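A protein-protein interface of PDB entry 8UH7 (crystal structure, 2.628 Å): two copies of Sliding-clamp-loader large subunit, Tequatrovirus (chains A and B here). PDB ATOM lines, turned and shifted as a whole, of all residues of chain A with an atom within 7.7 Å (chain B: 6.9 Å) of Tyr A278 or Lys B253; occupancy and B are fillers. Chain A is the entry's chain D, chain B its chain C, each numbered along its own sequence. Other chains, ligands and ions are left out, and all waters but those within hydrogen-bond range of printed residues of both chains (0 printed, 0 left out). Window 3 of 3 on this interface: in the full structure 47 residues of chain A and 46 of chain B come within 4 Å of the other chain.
The guanidinium group (NH2) of Arg B256 sits at hydrogen-bond distance from the backbone carbonyl oxygen (O) of Ala A274 (3.0 Å).
The guanidinium group (NE) of Arg B256 is in hydrogen-bond range of the side-chain hydroxyl (OH) of Tyr A290, 2.8 Å away.
Of the 10 printed residues of chain B, 4 touch a printed residue of chain A.
Printed residues of chain B that touch a printed residue of chain A: Val B252, Lys B253, Arg B256 and Ile B315.
Printed residues of chain A that touch a printed residue of chain B: Ala A274, Glu A275, Tyr A278 and Tyr A290.
Along chain A the printed residues that touch a printed residue of chain B span positions 274 to 290.
Among the printed residues, 7 pairs touch across the chains.
Among the printed residues, no Asp or Glu carboxylate lies within 4 Å of a Lys or Arg side-chain nitrogen of the other chain.
No position is printed for both chains.
Of the 7 pairs that touch across the chains among the printed residues, none has its exchanged pair printed and touching as well.
Of the printed residues of chain A, Lys B253 touches Tyr A278.
Of the printed residues of chain B, Tyr A290 touches Arg B256 (2.8 Å) and Ile B315 (3.9 Å).
Of the printed residues of chain A, Val B252 touches Tyr A278.
Of the printed residues of chain A, Ile B315 touches Tyr A290.
Printed residues of chain B within 4 Å of Ala A274: Arg B256.
The nearest printed residue of chain B that does not touch Tyr A278 is Ile B315 (6.3 Å).
The nearest printed residue of chain A that does not touch Lys B253 is Tyr A290 (7.7 Å).
Among the printed residues, pairs that only touch across the chains: Glu A275 with Arg B256, Tyr A278 with Val B252, Tyr A278 with Lys B253, Tyr A278 with Arg B256 and Tyr A290 with Ile B315.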
ATOM      1  N   LEU A 244      -9.190   1.194  -8.483  1.00  0.00           N
ATOM      2  CA  LEU A 244      -9.262   1.577  -9.891  1.00  0.00           C
ATOM      3  C   LEU A 244      -9.499   0.364 -10.786  1.00  0.00           C
ATOM      4  O   LEU A 244     -10.317   0.419 -11.715  1.00  0.00           O
ATOM      5  CB  LEU A 244      -7.985   2.308 -10.304  1.00  0.00           C
ATOM      6  CG  LEU A 244      -7.749   3.654  -9.612  1.00  0.00           C
ATOM      7  CD1 LEU A 244      -6.366   4.201  -9.932  1.00  0.00           C
ATOM      8  CD2 LEU A 244      -8.828   4.652  -9.995  1.00  0.00           C
ATOM      9  N   LYS A 272      -7.030  11.628  -3.729  1.00  0.00           N
ATOM     10  CA  LYS A 272      -6.200  10.701  -4.491  1.00  0.00           C
ATOM     11  C   LYS A 272      -6.976  10.086  -5.647  1.00  0.00           C
ATOM     12  O   LYS A 272      -6.417   9.845  -6.723  1.00  0.00           O
ATOM     13  CB  LYS A 272      -5.665   9.602  -3.574  1.00  0.00           C
ATOM     14  CG  LYS A 272      -4.152   9.569  -3.438  1.00  0.00           C
ATOM     15  CD  LYS A 272      -3.474   9.199  -4.744  1.00  0.00           C
ATOM     16  CE  LYS A 272      -1.962   9.173  -4.580  1.00  0.00           C
ATOM     17  NZ  LYS A 272      -1.262   8.919  -5.868  1.00  0.00           N
ATOM     18  N   LEU A 273      -8.270   9.833  -5.446  1.00  0.00           N
ATOM     19  CA  LEU A 273      -9.081   9.212  -6.481  1.00  0.00           C
ATOM     20  C   LEU A 273      -9.217  10.127  -7.685  1.00  0.00           C
ATOM     21  O   LEU A 273      -9.006   9.697  -8.822  1.00  0.00           O
ATOM     22  CB  LEU A 273     -10.458   8.845  -5.929  1.00  0.00           C
ATOM     23  CG  LEU A 273     -11.364   8.179  -6.962  1.00  0.00           C
ATOM     24  CD1 LEU A 273     -10.750   6.871  -7.439  1.00  0.00           C
ATOM     25  CD2 LEU A 273     -12.762   7.957  -6.407  1.00  0.00           C
ATOM     26  N   ALA A 274      -9.576  11.392  -7.462  1.00  0.00           N
ATOM     27  CA  ALA A 274      -9.608  12.332  -8.580  1.00  0.00           C
ATOM     28  C   ALA A 274      -8.238  12.420  -9.241  1.00  0.00           C
ATOM     29  O   ALA A 274      -8.107  12.241 -10.463  1.00  0.00           O
ATOM     30  CB  ALA A 274     -10.072  13.709  -8.104  1.00  0.00           C
ATOM     31  N   GLU A 275      -7.198  12.639  -8.423  1.00  0.00           N
ATOM     32  CA  GLU A 275      -5.840  12.831  -8.924  1.00  0.00           C
ATOM     33  C   GLU A 275      -5.389  11.681  -9.818  1.00  0.00           C
ATOM     34  O   GLU A 275      -4.731  11.902 -10.842  1.00  0.00           O
ATOM     35  CB  GLU A 275      -4.891  12.997  -7.737  1.00  0.00           C
ATOM     36  CG  GLU A 275      -3.451  13.317  -8.086  1.00  0.00           C
ATOM     37  CD  GLU A 275      -2.588  13.495  -6.846  1.00  0.00           C
ATOM     38  OE1 GLU A 275      -3.118  13.340  -5.724  1.00  0.00           O
ATOM     39  OE2 GLU A 275      -1.382  13.792  -6.990  1.00  0.00           O
ATOM     40  N   GLU A 276      -5.742  10.447  -9.457  1.00  0.00           N
ATOM     41  CA  GLU A 276      -5.288   9.278 -10.200  1.00  0.00           C
ATOM     42  C   GLU A 276      -6.213   8.926 -11.360  1.00  0.00           C
ATOM     43  O   GLU A 276      -5.747   8.724 -12.485  1.00  0.00           O
ATOM     44  CB  GLU A 276      -5.145   8.081  -9.255  1.00  0.00           C
ATOM     45  CG  GLU A 276      -3.936   8.165  -8.337  1.00  0.00           C
ATOM     46  CD  GLU A 276      -2.624   8.017  -9.086  1.00  0.00           C
ATOM     47  OE1 GLU A 276      -2.612   7.352 -10.143  1.00  0.00           O
ATOM     48  OE2 GLU A 276      -1.604   8.566  -8.617  1.00  0.00           O
ATOM     49  N   ILE A 277      -7.523   8.848 -11.112  1.00  0.00           N
ATOM     50  CA  ILE A 277      -8.468   8.436 -12.141  1.00  0.00           C
ATOM     51  C   ILE A 277      -8.635   9.467 -13.244  1.00  0.00           C
ATOM     52  O   ILE A 277      -9.250   9.157 -14.271  1.00  0.00           O
ATOM     53  CB  ILE A 277      -9.838   8.119 -11.509  1.00  0.00           C
ATOM     54  CG1 ILE A 277     -10.586   7.066 -12.324  1.00  0.00           C
ATOM     55  CG2 ILE A 277     -10.677   9.361 -11.424  1.00  0.00           C
ATOM     56  CD1 ILE A 277     -11.960   6.758 -11.782  1.00  0.00           C
ATOM     57  N   TYR A 278      -8.107  10.685 -13.077  1.00  0.00           N
ATOM     58  CA  TYR A 278      -8.067  11.595 -14.219  1.00  0.00           C
ATOM     59  C   TYR A 278      -7.334  10.981 -15.405  1.00  0.00           C
ATOM     60  O   TYR A 278      -7.637  11.305 -16.558  1.00  0.00           O
ATOM     61  CB  TYR A 278      -7.406  12.913 -13.817  1.00  0.00           C
ATOM     62  CG  TYR A 278      -7.262  13.915 -14.943  1.00  0.00           C
ATOM     63  CD1 TYR A 278      -8.329  14.713 -15.329  1.00  0.00           C
ATOM     64  CD2 TYR A 278      -6.051  14.075 -15.606  1.00  0.00           C
ATOM     65  CE1 TYR A 278      -8.201  15.633 -16.347  1.00  0.00           C
ATOM     66  CE2 TYR A 278      -5.912  14.997 -16.625  1.00  0.00           C
ATOM     67  CZ  TYR A 278      -6.991  15.773 -16.993  1.00  0.00           C
ATOM     68  OH  TYR A 278      -6.862  16.692 -18.012  1.00  0.00           O
ATOM     69  N   SER A 279      -6.379  10.086 -15.148  1.00  0.00           N
ATOM     70  CA  SER A 279      -5.536   9.529 -16.197  1.00  0.00           C
ATOM     71  C   SER A 279      -6.045   8.211 -16.760  1.00  0.00           C
ATOM     72  O   SER A 279      -5.612   7.816 -17.848  1.00  0.00           O
ATOM     73  CB  SER A 279      -4.108   9.320 -15.674  1.00  0.00           C
ATOM     74  OG  SER A 279      -4.057   8.286 -14.704  1.00  0.00           O
ATOM     75  N   ARG A 280      -6.941   7.522 -16.062  1.00  0.00           N
ATOM     76  CA  ARG A 280      -7.326   6.171 -16.439  1.00  0.00           C
ATOM     77  C   ARG A 280      -8.695   6.087 -17.097  1.00  0.00           C
ATOM     78  O   ARG A 280      -9.097   4.999 -17.520  1.00  0.00           O
ATOM     79  CB  ARG A 280      -7.277   5.260 -15.210  1.00  0.00           C
ATOM     80  CG  ARG A 280      -5.864   4.849 -14.844  1.00  0.00           C
ATOM     81  CD  ARG A 280      -5.629   4.921 -13.354  1.00  0.00           C
ATOM     82  NE  ARG A 280      -4.263   4.546 -13.007  1.00  0.00           N
ATOM     83  CZ  ARG A 280      -3.875   3.298 -12.770  1.00  0.00           C
ATOM     84  NH1 ARG A 280      -4.754   2.308 -12.844  1.00  0.00           N
ATOM     85  NH2 ARG A 280      -2.611   3.040 -12.462  1.00  0.00           N
ATOM     86  N   VAL A 281      -9.415   7.198 -17.206  1.00  0.00           N
ATOM     87  CA  VAL A 281     -10.699   7.226 -17.895  1.00  0.00           C
ATOM     88  C   VAL A 281     -10.538   8.013 -19.185  1.00  0.00           C
ATOM     89  O   VAL A 281      -9.648   8.862 -19.314  1.00  0.00           O
ATOM     90  CB  VAL A 281     -11.814   7.826 -17.016  1.00  0.00           C
ATOM     91  CG1 VAL A 281     -11.947   7.042 -15.722  1.00  0.00           C
ATOM     92  CG2 VAL A 281     -11.537   9.285 -16.728  1.00  0.00           C
ATOM     93  N   THR A 282     -11.404   7.718 -20.152  1.00  0.00           N
ATOM     94  CA  THR A 282     -11.343   8.391 -21.439  1.00  0.00           C
ATOM     95  C   THR A 282     -11.674   9.874 -21.275  1.00  0.00           C
ATOM     96  O   THR A 282     -12.418  10.252 -20.368  1.00  0.00           O
ATOM     97  CB  THR A 282     -12.312   7.747 -22.428  1.00  0.00           C
ATOM     98  OG1 THR A 282     -13.645   7.809 -21.906  1.00  0.00           O
ATOM     99  CG2 THR A 282     -11.935   6.293 -22.666  1.00  0.00           C
ATOM    100  N   PRO A 283     -11.126  10.732 -22.141  1.00  0.00           N
ATOM    101  CA  PRO A 283     -11.375  12.177 -21.999  1.00  0.00           C
ATOM    102  C   PRO A 283     -12.846  12.549 -22.010  1.00  0.00           C
ATOM    103  O   PRO A 283     -13.225  13.570 -21.423  1.00  0.00           O
ATOM    104  CB  PRO A 283     -10.633  12.776 -23.202  1.00  0.00           C
ATOM    105  CG  PRO A 283      -9.575  11.781 -23.522  1.00  0.00           C
ATOM    106  CD  PRO A 283     -10.188  10.442 -23.238  1.00  0.00           C
ATOM    107  N   ILE A 286     -14.348  12.769 -18.294  1.00  0.00           N
ATOM    108  CA  ILE A 286     -13.750  13.584 -17.240  1.00  0.00           C
ATOM    109  C   ILE A 286     -14.799  14.470 -16.578  1.00  0.00           C
ATOM    110  O   ILE A 286     -14.844  14.580 -15.349  1.00  0.00           O
ATOM    111  CB  ILE A 286     -12.571  14.407 -17.794  1.00  0.00           C
ATOM    112  CG1 ILE A 286     -11.252  13.668 -17.575  1.00  0.00           C
ATOM    113  CG2 ILE A 286     -12.493  15.774 -17.131  1.00  0.00           C
ATOM    114  CD1 ILE A 286     -11.120  12.404 -18.362  1.00  0.00           C
ATOM    115  N   ILE A 287     -15.658  15.113 -17.371  1.00  0.00           N
ATOM    116  CA  ILE A 287     -16.646  16.020 -16.792  1.00  0.00           C
ATOM    117  C   ILE A 287     -17.629  15.250 -15.919  1.00  0.00           C
ATOM    118  O   ILE A 287     -17.970  15.684 -14.813  1.00  0.00           O
ATOM    119  CB  ILE A 287     -17.368  16.810 -17.896  1.00  0.00           C
ATOM    120  CG1 ILE A 287     -16.357  17.513 -18.799  1.00  0.00           C
ATOM    121  CG2 ILE A 287     -18.307  17.832 -17.285  1.00  0.00           C
ATOM    122  CD1 ILE A 287     -16.996  18.214 -19.979  1.00  0.00           C
ATOM    123  N   MET A 289     -17.089  12.333 -14.444  1.00  0.00           N
ATOM    124  CA  MET A 289     -16.402  11.824 -13.264  1.00  0.00           C
ATOM    125  C   MET A 289     -16.160  12.928 -12.249  1.00  0.00           C
ATOM    126  O   MET A 289     -16.222  12.678 -11.040  1.00  0.00           O
ATOM    127  CB  MET A 289     -15.091  11.154 -13.670  1.00  0.00           C
ATOM    128  CG  MET A 289     -13.881  12.057 -13.653  1.00  0.00           C
ATOM    129  SD  MET A 289     -12.905  11.771 -12.176  1.00  0.00           S
ATOM    130  CE  MET A 289     -12.638  13.430 -11.582  1.00  0.00           C
ATOM    131  N   TYR A 290     -15.918  14.158 -12.713  1.00  0.00           N
ATOM    132  CA  TYR A 290     -15.792  15.265 -11.776  1.00  0.00           C
ATOM    133  C   TYR A 290     -17.134  15.594 -11.150  1.00  0.00           C
ATOM    134  O   TYR A 290     -17.200  15.893  -9.960  1.00  0.00           O
ATOM    135  CB  TYR A 290     -15.187  16.495 -12.452  1.00  0.00           C
ATOM    136  CG  TYR A 290     -13.720  16.660 -12.127  1.00  0.00           C
ATOM    137  CD1 TYR A 290     -13.308  16.939 -10.832  1.00  0.00           C
ATOM    138  CD2 TYR A 290     -12.746  16.511 -13.109  1.00  0.00           C
ATOM    139  CE1 TYR A 290     -11.965  17.075 -10.521  1.00  0.00           C
ATOM    140  CE2 TYR A 290     -11.400  16.644 -12.808  1.00  0.00           C
ATOM    141  CZ  TYR A 290     -11.018  16.928 -11.512  1.00  0.00           C
ATOM    142  OH  TYR A 290      -9.685  17.065 -11.204  1.00  0.00           O
ATOM    143  N   TRP A 323     -13.334   3.549 -19.862  1.00  0.00           N
ATOM    144  CA  TRP A 323     -11.937   3.407 -19.487  1.00  0.00           C
ATOM    145  C   TRP A 323     -11.049   3.262 -20.716  1.00  0.00           C
ATOM    146  O   TRP A 323     -11.481   2.782 -21.768  1.00  0.00           O
ATOM    147  CB  TRP A 323     -11.756   2.205 -18.559  1.00  0.00           C
ATOM    148  CG  TRP A 323     -12.643   2.270 -17.360  1.00  0.00           C
ATOM    149  CD1 TRP A 323     -13.938   1.847 -17.273  1.00  0.00           C
ATOM    150  CD2 TRP A 323     -12.311   2.809 -16.076  1.00  0.00           C
ATOM    151  NE1 TRP A 323     -14.431   2.082 -16.012  1.00  0.00           N
ATOM    152  CE2 TRP A 323     -13.451   2.672 -15.258  1.00  0.00           C
ATOM    153  CE3 TRP A 323     -11.159   3.390 -15.538  1.00  0.00           C
ATOM    154  CZ2 TRP A 323     -13.470   3.094 -13.932  1.00  0.00           C
ATOM    155  CZ3 TRP A 323     -11.181   3.807 -14.222  1.00  0.00           C
ATOM    156  CH2 TRP A 323     -12.330   3.658 -13.434  1.00  0.00           C
ATOM    157  N   LYS A 324      -9.800   3.691 -20.567  1.00  0.00           N
ATOM    158  CA  LYS A 324      -8.803   3.571 -21.622  1.00  0.00           C
ATOM    159  C   LYS A 324      -7.888   2.383 -21.342  1.00  0.00           C
ATOM    160  O   LYS A 324      -7.233   1.850 -22.239  1.00  0.00           O
ATOM    161  CB  LYS A 324      -7.986   4.860 -21.738  1.00  0.00           C
ATOM    162  CG  LYS A 324      -7.421   5.340 -20.411  1.00  0.00           C
ATOM    163  CD  LYS A 324      -6.281   6.334 -20.591  1.00  0.00           C
ATOM    164  CE  LYS A 324      -6.764   7.691 -21.063  1.00  0.00           C
ATOM    165  NZ  LYS A 324      -5.662   8.695 -21.014  1.00  0.00           N
ATOM    166  OXT LYS A 324      -7.781   1.925 -20.204  1.00  0.00           O
ATOM    167  N   LYS B 250      -9.324  27.014 -20.788  1.00  0.00           N
ATOM    168  CA  LYS B 250      -9.772  25.654 -20.480  1.00  0.00           C
ATOM    169  C   LYS B 250      -8.589  24.755 -20.126  1.00  0.00           C
ATOM    170  O   LYS B 250      -8.538  23.584 -20.509  1.00  0.00           O
ATOM    171  CB  LYS B 250     -10.585  25.052 -21.631  1.00  0.00           C
ATOM    172  CG  LYS B 250     -11.853  25.814 -21.974  1.00  0.00           C
ATOM    173  CD  LYS B 250     -12.694  25.052 -22.989  1.00  0.00           C
ATOM    174  CE  LYS B 250     -13.991  25.788 -23.287  1.00  0.00           C
ATOM    175  NZ  LYS B 250     -14.884  24.999 -24.184  1.00  0.00           N
ATOM    176  N   ASP B 251      -7.625  25.308 -19.391  1.00  0.00           N
ATOM    177  CA  ASP B 251      -6.443  24.559 -18.963  1.00  0.00           C
ATOM    178  C   ASP B 251      -6.808  23.757 -17.721  1.00  0.00           C
ATOM    179  O   ASP B 251      -6.594  24.189 -16.587  1.00  0.00           O
ATOM    180  CB  ASP B 251      -5.274  25.499 -18.695  1.00  0.00           C
ATOM    181  CG  ASP B 251      -3.935  24.782 -18.704  1.00  0.00           C
ATOM    182  OD1 ASP B 251      -2.996  25.283 -19.357  1.00  0.00           O
ATOM    183  OD2 ASP B 251      -3.825  23.710 -18.070  1.00  0.00           O
ATOM    184  N   VAL B 252      -7.361  22.562 -17.941  1.00  0.00           N
ATOM    185  CA  VAL B 252      -7.846  21.739 -16.835  1.00  0.00           C
ATOM    186  C   VAL B 252      -6.715  21.399 -15.872  1.00  0.00           C
ATOM    187  O   VAL B 252      -6.875  21.493 -14.650  1.00  0.00           O
ATOM    188  CB  VAL B 252      -8.529  20.472 -17.381  1.00  0.00           C
ATOM    189  CG1 VAL B 252      -8.619  19.411 -16.303  1.00  0.00           C
ATOM    190  CG2 VAL B 252      -9.907  20.811 -17.914  1.00  0.00           C
ATOM    191  N   LYS B 253      -5.555  21.008 -16.405  1.00  0.00           N
ATOM    192  CA  LYS B 253      -4.443  20.614 -15.545  1.00  0.00           C
ATOM    193  C   LYS B 253      -3.963  21.780 -14.688  1.00  0.00           C
ATOM    194  O   LYS B 253      -3.674  21.610 -13.495  1.00  0.00           O
ATOM    195  CB  LYS B 253      -3.301  20.063 -16.398  1.00  0.00           C
ATOM    196  CG  LYS B 253      -3.761  19.142 -17.518  1.00  0.00           C
ATOM    197  CD  LYS B 253      -2.588  18.426 -18.161  1.00  0.00           C
ATOM    198  CE  LYS B 253      -3.027  17.601 -19.363  1.00  0.00           C
ATOM    199  NZ  LYS B 253      -3.443  18.461 -20.507  1.00  0.00           N
ATOM    200  N   GLN B 254      -3.881  22.978 -15.275  1.00  0.00           N
ATOM    201  CA  GLN B 254      -3.469  24.147 -14.505  1.00  0.00           C
ATOM    202  C   GLN B 254      -4.459  24.440 -13.387  1.00  0.00           C
ATOM    203  O   GLN B 254      -4.062  24.824 -12.285  1.00  0.00           O
ATOM    204  CB  GLN B 254      -3.320  25.362 -15.419  1.00  0.00           C
ATOM    205  CG  GLN B 254      -2.834  26.623 -14.720  1.00  0.00           C
ATOM    206  CD  GLN B 254      -1.329  26.650 -14.502  1.00  0.00           C
ATOM    207  OE1 GLN B 254      -0.639  25.647 -14.690  1.00  0.00           O
ATOM    208  NE2 GLN B 254      -0.815  27.811 -14.106  1.00  0.00           N
ATOM    209  N   LEU B 255      -5.756  24.255 -13.649  1.00  0.00           N
ATOM    210  CA  LEU B 255      -6.754  24.487 -12.609  1.00  0.00           C
ATOM    211  C   LEU B 255      -6.638  23.454 -11.494  1.00  0.00           C
ATOM    212  O   LEU B 255      -6.785  23.787 -10.307  1.00  0.00           O
ATOM    213  CB  LEU B 255      -8.151  24.471 -13.225  1.00  0.00           C
ATOM    214  CG  LEU B 255      -8.375  25.553 -14.280  1.00  0.00           C
ATOM    215  CD1 LEU B 255      -9.603  25.244 -15.117  1.00  0.00           C
ATOM    216  CD2 LEU B 255      -8.501  26.917 -13.620  1.00  0.00           C
ATOM    217  N   ARG B 256      -6.380  22.195 -11.857  1.00  0.00           N
ATOM    218  CA  ARG B 256      -6.133  21.178 -10.843  1.00  0.00           C
ATOM    219  C   ARG B 256      -4.926  21.544  -9.991  1.00  0.00           C
ATOM    220  O   ARG B 256      -4.903  21.276  -8.784  1.00  0.00           O
ATOM    221  CB  ARG B 256      -5.925  19.814 -11.498  1.00  0.00           C
ATOM    222  CG  ARG B 256      -7.035  19.385 -12.433  1.00  0.00           C
ATOM    223  CD  ARG B 256      -6.693  18.055 -13.069  1.00  0.00           C
ATOM    224  NE  ARG B 256      -7.032  16.941 -12.193  1.00  0.00           N
ATOM    225  CZ  ARG B 256      -6.371  15.791 -12.159  1.00  0.00           C
ATOM    226  NH1 ARG B 256      -5.317  15.612 -12.942  1.00  0.00           N
ATOM    227  NH2 ARG B 256      -6.754  14.827 -11.333  1.00  0.00           N
ATOM    228  N   ALA B 257      -3.914  22.161 -10.605  1.00  0.00           N
ATOM    229  CA  ALA B 257      -2.751  22.600  -9.838  1.00  0.00           C
ATOM    230  C   ALA B 257      -3.060  23.829  -8.990  1.00  0.00           C
ATOM    231  O   ALA B 257      -2.458  24.018  -7.928  1.00  0.00           O
ATOM    232  CB  ALA B 257      -1.581  22.896 -10.773  1.00  0.00           C
ATOM    233  N   LEU B 258      -3.984  24.675  -9.442  1.00  0.00           N
ATOM    234  CA  LEU B 258      -4.245  25.945  -8.781  1.00  0.00           C
ATOM    235  C   LEU B 258      -5.229  25.833  -7.628  1.00  0.00           C
ATOM    236  O   LEU B 258      -5.258  26.731  -6.779  1.00  0.00           O
ATOM    237  CB  LEU B 258      -4.776  26.963  -9.791  1.00  0.00           C
ATOM    238  CG  LEU B 258      -3.751  27.602 -10.724  1.00  0.00           C
ATOM    239  CD1 LEU B 258      -4.458  28.466 -11.752  1.00  0.00           C
ATOM    240  CD2 LEU B 258      -2.750  28.414  -9.917  1.00  0.00           C
ATOM    241  N   ILE B 315     -13.453  23.065 -12.925  1.00  0.00           N
ATOM    242  CA  ILE B 315     -13.806  22.274 -14.102  1.00  0.00           C
ATOM    243  C   ILE B 315     -15.162  22.702 -14.644  1.00  0.00           C
ATOM    244  O   ILE B 315     -15.333  22.884 -15.857  1.00  0.00           O
ATOM    245  CB  ILE B 315     -13.783  20.772 -13.775  1.00  0.00           C
ATOM    246  CG1 ILE B 315     -12.352  20.319 -13.517  1.00  0.00           C
ATOM    247  CG2 ILE B 315     -14.388  19.976 -14.918  1.00  0.00           C
ATOM    248  CD1 ILE B 315     -11.405  20.749 -14.603  1.00  0.00           C
